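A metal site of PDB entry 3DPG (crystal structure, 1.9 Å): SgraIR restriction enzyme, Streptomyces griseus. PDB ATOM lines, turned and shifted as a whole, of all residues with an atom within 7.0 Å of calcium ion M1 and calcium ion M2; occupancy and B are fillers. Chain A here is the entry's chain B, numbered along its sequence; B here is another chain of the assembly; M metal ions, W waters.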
ATOM      1  N   GLY A  98     -19.978 -20.099   0.707  1.00  0.00           N
ATOM      2  CA  GLY A  98     -19.007 -19.679   1.704  1.00  0.00           C
ATOM      3  C   GLY A  98     -17.965 -20.761   1.931  1.00  0.00           C
ATOM      4  O   GLY A  98     -16.770 -20.497   1.916  1.00  0.00           O
ATOM      5  N   GLU A 102     -13.796 -20.694   0.968  1.00  0.00           N
ATOM      6  CA  GLU A 102     -12.776 -20.995   1.952  1.00  0.00           C
ATOM      7  C   GLU A 102     -11.952 -22.224   1.562  1.00  0.00           C
ATOM      8  O   GLU A 102     -10.726 -22.172   1.538  1.00  0.00           O
ATOM      9  CB  GLU A 102     -13.411 -21.227   3.323  1.00  0.00           C
ATOM     10  CG  GLU A 102     -12.525 -22.012   4.237  1.00  0.00           C
ATOM     11  CD  GLU A 102     -12.918 -21.858   5.667  1.00  0.00           C
ATOM     12  OE1 GLU A 102     -14.071 -21.479   5.964  1.00  0.00           O
ATOM     13  OE2 GLU A 102     -12.029 -22.085   6.497  1.00  0.00           O
ATOM     14  N   SER A 106      -8.111 -22.217   0.339  1.00  0.00           N
ATOM     15  CA  SER A 106      -7.181 -22.934   1.214  1.00  0.00           C
ATOM     16  C   SER A 106      -6.368 -23.975   0.455  1.00  0.00           C
ATOM     17  O   SER A 106      -5.191 -24.196   0.740  1.00  0.00           O
ATOM     18  CB  SER A 106      -7.942 -23.615   2.353  1.00  0.00           C
ATOM     19  OG  SER A 106      -8.663 -22.654   3.107  1.00  0.00           O
ATOM     20  N   LEU A 147      -2.877 -24.562   7.273  1.00  0.00           N
ATOM     21  CA  LEU A 147      -3.833 -25.285   8.098  1.00  0.00           C
ATOM     22  C   LEU A 147      -5.219 -24.684   8.026  1.00  0.00           C
ATOM     23  O   LEU A 147      -5.487 -23.633   8.608  1.00  0.00           O
ATOM     24  CB  LEU A 147      -3.382 -25.325   9.556  1.00  0.00           C
ATOM     25  CG  LEU A 147      -1.936 -25.729   9.875  1.00  0.00           C
ATOM     26  CD1 LEU A 147      -1.736 -25.835  11.376  1.00  0.00           C
ATOM     27  CD2 LEU A 147      -1.589 -27.053   9.179  1.00  0.00           C
ATOM     28  N   ASN A 148      -6.098 -25.352   7.295  1.00  0.00           N
ATOM     29  CA  ASN A 148      -7.522 -25.040   7.326  1.00  0.00           C
ATOM     30  C   ASN A 148      -8.057 -25.470   8.699  1.00  0.00           C
ATOM     31  O   ASN A 148      -8.148 -26.662   8.995  1.00  0.00           O
ATOM     32  CB  ASN A 148      -8.224 -25.772   6.189  1.00  0.00           C
ATOM     33  CG  ASN A 148      -9.703 -25.484   6.144  1.00  0.00           C
ATOM     34  OD1 ASN A 148     -10.220 -24.850   7.039  1.00  0.00           O
ATOM     35  ND2 ASN A 148     -10.391 -25.932   5.092  1.00  0.00           N
ATOM     36  N   LEU A 149      -8.404 -24.501   9.549  1.00  0.00           N
ATOM     37  CA  LEU A 149      -8.780 -24.813  10.929  1.00  0.00           C
ATOM     38  C   LEU A 149     -10.255 -25.202  11.041  1.00  0.00           C
ATOM     39  O   LEU A 149     -11.079 -24.696  10.310  1.00  0.00           O
ATOM     40  CB  LEU A 149      -8.433 -23.637  11.838  1.00  0.00           C
ATOM     41  CG  LEU A 149      -6.961 -23.234  11.728  1.00  0.00           C
ATOM     42  CD1 LEU A 149      -6.645 -22.050  12.629  1.00  0.00           C
ATOM     43  CD2 LEU A 149      -6.076 -24.420  12.057  1.00  0.00           C
ATOM     44  N   PRO A 150     -10.600 -26.131  11.949  1.00  0.00           N
ATOM     45  CA  PRO A 150     -11.981 -26.619  11.938  1.00  0.00           C
ATOM     46  C   PRO A 150     -12.957 -25.807  12.791  1.00  0.00           C
ATOM     47  O   PRO A 150     -12.547 -24.887  13.501  1.00  0.00           O
ATOM     48  CB  PRO A 150     -11.839 -28.018  12.502  1.00  0.00           C
ATOM     49  CG  PRO A 150     -10.754 -27.854  13.521  1.00  0.00           C
ATOM     50  CD  PRO A 150      -9.775 -26.839  12.937  1.00  0.00           C
ATOM     51  N   ARG A 151     -14.238 -26.137  12.719  1.00  0.00           N
ATOM     52  CA  ARG A 151     -15.220 -25.514  13.595  1.00  0.00           C
ATOM     53  C   ARG A 151     -14.860 -25.817  15.048  1.00  0.00           C
ATOM     54  O   ARG A 151     -14.282 -26.859  15.352  1.00  0.00           O
ATOM     55  CB  ARG A 151     -16.623 -26.027  13.291  1.00  0.00           C
ATOM     56  CG  ARG A 151     -16.963 -27.353  13.965  1.00  0.00           C
ATOM     57  CD  ARG A 151     -18.401 -27.767  13.681  1.00  0.00           C
ATOM     58  NE  ARG A 151     -18.662 -29.132  14.120  1.00  0.00           N
ATOM     59  CZ  ARG A 151     -19.205 -29.438  15.299  1.00  0.00           C
ATOM     60  NH1 ARG A 151     -19.540 -28.481  16.149  1.00  0.00           N
ATOM     61  NH2 ARG A 151     -19.401 -30.711  15.627  1.00  0.00           N
ATOM     62  N   THR A 185     -10.872 -18.607  16.457  1.00  0.00           N
ATOM     63  CA  THR A 185      -9.976 -19.101  15.424  1.00  0.00           C
ATOM     64  C   THR A 185     -10.145 -18.329  14.132  1.00  0.00           C
ATOM     65  O   THR A 185     -11.268 -17.959  13.769  1.00  0.00           O
ATOM     66  CB  THR A 185     -10.223 -20.606  15.131  1.00  0.00           C
ATOM     67  OG1 THR A 185      -9.185 -21.125  14.288  1.00  0.00           O
ATOM     68  CG2 THR A 185     -11.582 -20.824  14.461  1.00  0.00           C
ATOM     69  N   PRO A 186      -9.036 -18.080  13.419  1.00  0.00           N
ATOM     70  CA  PRO A 186      -9.180 -17.654  12.024  1.00  0.00           C
ATOM     71  C   PRO A 186      -9.639 -18.863  11.202  1.00  0.00           C
ATOM     72  O   PRO A 186      -9.645 -19.976  11.733  1.00  0.00           O
ATOM     73  CB  PRO A 186      -7.766 -17.237  11.642  1.00  0.00           C
ATOM     74  CG  PRO A 186      -6.864 -18.039  12.550  1.00  0.00           C
ATOM     75  CD  PRO A 186      -7.629 -18.258  13.824  1.00  0.00           C
ATOM     76  N   ASP A 187     -10.016 -18.660   9.941  1.00  0.00           N
ATOM     77  CA  ASP A 187     -10.393 -19.793   9.094  1.00  0.00           C
ATOM     78  C   ASP A 187      -9.190 -20.676   8.856  1.00  0.00           C
ATOM     79  O   ASP A 187      -9.297 -21.889   8.688  1.00  0.00           O
ATOM     80  CB  ASP A 187     -10.866 -19.290   7.736  1.00  0.00           C
ATOM     81  CG  ASP A 187     -12.257 -18.750   7.769  1.00  0.00           C
ATOM     82  OD1 ASP A 187     -13.081 -19.272   8.545  1.00  0.00           O
ATOM     83  OD2 ASP A 187     -12.516 -17.785   7.030  1.00  0.00           O
ATOM     84  N   LEU A 188      -8.045 -20.031   8.814  1.00  0.00           N
ATOM     85  CA  LEU A 188      -6.849 -20.693   8.329  1.00  0.00           C
ATOM     86  C   LEU A 188      -5.657 -20.056   8.982  1.00  0.00           C
ATOM     87  O   LEU A 188      -5.637 -18.845   9.213  1.00  0.00           O
ATOM     88  CB  LEU A 188      -6.784 -20.563   6.795  1.00  0.00           C
ATOM     89  CG  LEU A 188      -5.542 -21.054   6.029  1.00  0.00           C
ATOM     90  CD1 LEU A 188      -5.918 -21.420   4.600  1.00  0.00           C
ATOM     91  CD2 LEU A 188      -4.438 -20.011   6.021  1.00  0.00           C
ATOM     92  N   VAL A 238      -5.766 -16.169   8.166  1.00  0.00           N
ATOM     93  CA  VAL A 238      -6.651 -15.673   7.125  1.00  0.00           C
ATOM     94  C   VAL A 238      -8.103 -15.910   7.521  1.00  0.00           C
ATOM     95  O   VAL A 238      -8.450 -16.968   8.073  1.00  0.00           O
ATOM     96  CB  VAL A 238      -6.368 -16.348   5.754  1.00  0.00           C
ATOM     97  CG1 VAL A 238      -7.352 -15.842   4.685  1.00  0.00           C
ATOM     98  CG2 VAL A 238      -4.916 -16.106   5.328  1.00  0.00           C
ATOM     99  N   ALA A 239      -8.944 -14.914   7.253  1.00  0.00           N
ATOM    100  CA  ALA A 239     -10.399 -15.059   7.336  1.00  0.00           C
ATOM    101  C   ALA A 239     -11.031 -14.868   5.948  1.00  0.00           C
ATOM    102  O   ALA A 239     -10.818 -13.842   5.302  1.00  0.00           O
ATOM    103  CB  ALA A 239     -10.993 -14.052   8.316  1.00  0.00           C
ATOM    104  N   PHE A 240     -11.806 -15.851   5.512  1.00  0.00           N
ATOM    105  CA  PHE A 240     -12.497 -15.778   4.230  1.00  0.00           C
ATOM    106  C   PHE A 240     -13.938 -15.359   4.439  1.00  0.00           C
ATOM    107  O   PHE A 240     -14.627 -15.918   5.279  1.00  0.00           O
ATOM    108  CB  PHE A 240     -12.460 -17.144   3.518  1.00  0.00           C
ATOM    109  CG  PHE A 240     -11.056 -17.650   3.247  1.00  0.00           C
ATOM    110  CD1 PHE A 240     -10.306 -17.113   2.216  1.00  0.00           C
ATOM    111  CD2 PHE A 240     -10.499 -18.633   4.036  1.00  0.00           C
ATOM    112  CE1 PHE A 240      -9.008 -17.561   1.971  1.00  0.00           C
ATOM    113  CE2 PHE A 240      -9.201 -19.089   3.796  1.00  0.00           C
ATOM    114  CZ  PHE A 240      -8.460 -18.546   2.757  1.00  0.00           C
ATOM    115  N   LYS A 241     -14.388 -14.359   3.702  1.00  0.00           N
ATOM    116  CA  LYS A 241     -15.806 -14.019   3.703  1.00  0.00           C
ATOM    117  C   LYS A 241     -16.174 -13.714   2.271  1.00  0.00           C
ATOM    118  O   LYS A 241     -15.737 -12.703   1.730  1.00  0.00           O
ATOM    119  CB  LYS A 241     -16.071 -12.785   4.579  1.00  0.00           C
ATOM    120  CG  LYS A 241     -15.796 -13.000   6.048  1.00  0.00           C
ATOM    121  CD  LYS A 241     -15.888 -11.700   6.856  1.00  0.00           C
ATOM    122  CE  LYS A 241     -15.777 -11.993   8.339  1.00  0.00           C
ATOM    123  NZ  LYS A 241     -16.991 -12.672   8.867  1.00  0.00           N
ATOM    124  N   ARG A 242     -16.967 -14.592   1.649  1.00  0.00           N
ATOM    125  CA  ARG A 242     -17.199 -14.473   0.202  1.00  0.00           C
ATOM    126  C   ARG A 242     -17.735 -13.100  -0.180  1.00  0.00           C
ATOM    127  O   ARG A 242     -17.346 -12.539  -1.204  1.00  0.00           O
ATOM    128  CB  ARG A 242     -18.141 -15.580  -0.308  1.00  0.00           C
ATOM    129  CG  ARG A 242     -17.933 -15.909  -1.796  1.00  0.00           C
ATOM    130  CD  ARG A 242     -19.217 -16.431  -2.429  1.00  0.00           C
ATOM    131  NE  ARG A 242     -20.212 -15.374  -2.473  1.00  0.00           N
ATOM    132  CZ  ARG A 242     -20.221 -14.386  -3.356  1.00  0.00           C
ATOM    133  NH1 ARG A 242     -19.287 -14.318  -4.301  1.00  0.00           N
ATOM    134  NH2 ARG A 242     -21.154 -13.447  -3.301  1.00  0.00           N
ATOM    135  N   GLN A 251     -15.591 -10.278  13.514  1.00  0.00           N
ATOM    136  CA  GLN A 251     -14.967 -11.463  14.095  1.00  0.00           C
ATOM    137  C   GLN A 251     -13.453 -11.526  13.831  1.00  0.00           C
ATOM    138  O   GLN A 251     -12.688 -11.782  14.753  1.00  0.00           O
ATOM    139  CB  GLN A 251     -15.674 -12.761  13.661  1.00  0.00           C
ATOM    140  CG  GLN A 251     -15.154 -14.019  14.360  1.00  0.00           C
ATOM    141  CD  GLN A 251     -13.876 -14.569  13.706  1.00  0.00           C
ATOM    142  OE1 GLN A 251     -13.631 -14.334  12.525  1.00  0.00           O
ATOM    143  NE2 GLN A 251     -13.078 -15.301  14.476  1.00  0.00           N
ATOM    144  N   PRO A 252     -13.025 -11.266  12.576  1.00  0.00           N
ATOM    145  CA  PRO A 252     -11.580 -11.284  12.301  1.00  0.00           C
ATOM    146  C   PRO A 252     -10.886 -10.112  12.961  1.00  0.00           C
ATOM    147  O   PRO A 252      -9.746 -10.245  13.428  1.00  0.00           O
ATOM    148  CB  PRO A 252     -11.502 -11.124  10.778  1.00  0.00           C
ATOM    149  CG  PRO A 252     -12.826 -11.550  10.268  1.00  0.00           C
ATOM    150  CD  PRO A 252     -13.817 -11.194  11.338  1.00  0.00           C
ATOM    151  P    DA B   7     -17.414 -22.016  15.445  1.00  0.00           P
ATOM    152  OP1  DA B   7     -15.955 -22.244  15.361  1.00  0.00           O
ATOM    153  OP2  DA B   7     -17.972 -21.069  16.444  1.00  0.00           O
ATOM    154  O5'  DA B   7     -17.923 -21.566  14.002  1.00  0.00           O
ATOM    155  C5'  DA B   7     -17.466 -22.287  12.864  1.00  0.00           C
ATOM    156  C4'  DA B   7     -18.170 -21.770  11.635  1.00  0.00           C
ATOM    157  O4'  DA B   7     -19.580 -22.084  11.738  1.00  0.00           O
ATOM    158  C3'  DA B   7     -18.092 -20.256  11.423  1.00  0.00           C
ATOM    159  O3'  DA B   7     -17.613 -20.099  10.107  1.00  0.00           O
ATOM    160  C2'  DA B   7     -19.530 -19.778  11.594  1.00  0.00           C
ATOM    161  C1'  DA B   7     -20.291 -21.024  11.162  1.00  0.00           C
ATOM    162  N9   DA B   7     -21.635 -21.176  11.695  1.00  0.00           N
ATOM    163  C8   DA B   7     -22.073 -20.811  12.931  1.00  0.00           C
ATOM    164  N7   DA B   7     -23.332 -21.106  13.146  1.00  0.00           N
ATOM    165  C5   DA B   7     -23.743 -21.703  11.964  1.00  0.00           C
ATOM    166  C6   DA B   7     -24.967 -22.232  11.561  1.00  0.00           C
ATOM    167  N6   DA B   7     -26.052 -22.230  12.346  1.00  0.00           N
ATOM    168  N1   DA B   7     -25.056 -22.765  10.319  1.00  0.00           N
ATOM    169  C2   DA B   7     -23.957 -22.759   9.548  1.00  0.00           C
ATOM    170  N3   DA B   7     -22.739 -22.293   9.821  1.00  0.00           N
ATOM    171  C4   DA B   7     -22.701 -21.771  11.060  1.00  0.00           C
ATOM    172  P    DC B   8     -17.362 -18.694   9.401  1.00  0.00           P
ATOM    173  OP1  DC B   8     -15.963 -18.722   8.927  1.00  0.00           O
ATOM    174  OP2  DC B   8     -17.803 -17.585  10.292  1.00  0.00           O
ATOM    175  O5'  DC B   8     -18.361 -18.782   8.160  1.00  0.00           O
ATOM    176  C5'  DC B   8     -18.129 -19.754   7.153  1.00  0.00           C
ATOM    177  C4'  DC B   8     -19.324 -19.841   6.223  1.00  0.00           C
ATOM    178  O4'  DC B   8     -20.443 -20.448   6.903  1.00  0.00           O
ATOM    179  C3'  DC B   8     -19.859 -18.502   5.735  1.00  0.00           C
ATOM    180  O3'  DC B   8     -19.119 -18.128   4.603  1.00  0.00           O
ATOM    181  C2'  DC B   8     -21.302 -18.865   5.347  1.00  0.00           C
ATOM    182  C1'  DC B   8     -21.651 -19.957   6.352  1.00  0.00           C
ATOM    183  N1   DC B   8     -22.494 -19.498   7.499  1.00  0.00           N
ATOM    184  C2   DC B   8     -23.876 -19.647   7.437  1.00  0.00           C
ATOM    185  O2   DC B   8     -24.400 -20.144   6.432  1.00  0.00           O
ATOM    186  N3   DC B   8     -24.626 -19.249   8.501  1.00  0.00           N
ATOM    187  C4   DC B   8     -24.050 -18.706   9.578  1.00  0.00           C
ATOM    188  N4   DC B   8     -24.840 -18.331  10.586  1.00  0.00           N
ATOM    189  C5   DC B   8     -22.630 -18.542   9.647  1.00  0.00           C
ATOM    190  C6   DC B   8     -21.907 -18.942   8.598  1.00  0.00           C
ATOM    191  P    DC B   9     -18.992 -16.603   4.158  1.00  0.00           P
ATOM    192  OP1  DC B   9     -18.021 -16.589   3.046  1.00  0.00           O
ATOM    193  OP2  DC B   9     -18.795 -15.782   5.371  1.00  0.00           O
ATOM    194  O5'  DC B   9     -20.452 -16.225   3.617  1.00  0.00           O
ATOM    195  C5'  DC B   9     -21.015 -16.932   2.529  1.00  0.00           C
ATOM    196  C4'  DC B   9     -22.416 -16.391   2.256  1.00  0.00           C
ATOM    197  O4'  DC B   9     -23.228 -16.592   3.443  1.00  0.00           O
ATOM    198  C3'  DC B   9     -22.506 -14.903   1.955  1.00  0.00           C
ATOM    199  O3'  DC B   9     -23.585 -14.704   1.067  1.00  0.00           O
ATOM    200  C2'  DC B   9     -22.853 -14.270   3.312  1.00  0.00           C
ATOM    201  C1'  DC B   9     -23.743 -15.360   3.899  1.00  0.00           C
ATOM    202  N1   DC B   9     -23.821 -15.389   5.385  1.00  0.00           N
ATOM    203  C2   DC B   9     -25.081 -15.394   6.000  1.00  0.00           C
ATOM    204  O2   DC B   9     -26.111 -15.377   5.312  1.00  0.00           O
ATOM    205  N3   DC B   9     -25.152 -15.422   7.344  1.00  0.00           N
ATOM    206  C4   DC B   9     -24.042 -15.435   8.080  1.00  0.00           C
ATOM    207  N4   DC B   9     -24.185 -15.456   9.410  1.00  0.00           N
ATOM    208  C5   DC B   9     -22.746 -15.432   7.483  1.00  0.00           C
ATOM    209  C6   DC B   9     -22.684 -15.406   6.136  1.00  0.00           C
HETATM  210 CA    CA M   1     -11.560 -23.286   8.505  1.00  0.00          CA
HETATM  211 CA    CA M   2     -14.864 -17.315   7.280  1.00  0.00          CA
HETATM  212  O   HOH W   1     -17.033 -16.159   7.311  1.00  0.00           O
HETATM  213  O   HOH W   2     -13.397 -24.938   8.191  1.00  0.00           O
HETATM  214  O   HOH W   3     -14.137 -15.537   8.816  1.00  0.00           O
HETATM  215  O   HOH W   4     -13.012 -21.837   9.918  1.00  0.00           O
HETATM  216  O   HOH W   5     -15.237 -19.103   5.540  1.00  0.00           O
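OG of Ser 106 lies within hydrogen-bond range of O of Glu 102, 2.6 Å away.
The backbone NH of Asp 187 sits at hydrogen-bond distance from the backbone carbonyl oxygen of Val 238 (3.0 Å).
Of the 22 residues printed, 4 come within 4 Å of calcium ion M1.
The side-chain carboxylate (OD2) of Asp 187 is bound to calcium ion M2 (2.4 Å).
OP1 of DC 8 of chain B is bound to calcium ion M2.
The backbone carbonyl oxygen (O) of Phe 240 is bound to calcium ion M2, at 2.5 Å.
Calcium ion M2 is bound by water W1 (2.5 Å).
Calcium ion M2 is bound by water W3, at 2.5 Å.
Water W5 is bound to calcium ion M2 (2.5 Å).
Slightly farther from calcium ion M2 lies the side-chain carboxylate (OD1) of Asp 187 (2.9 Å).
Three residues have an atom within 4 Å of calcium ion M2: Asp 187, Phe 240 and DC 8 of chain B.
Calcium ion M1 is bound by the backbone carbonyl oxygen (O) of Leu 149, the side-chain carboxylate (OE2) of Glu 102, water W2, water W4, the side-chain amide oxygen (OD1) of Asn 148 and the backbone carbonyl oxygen (O) of Asp 187.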
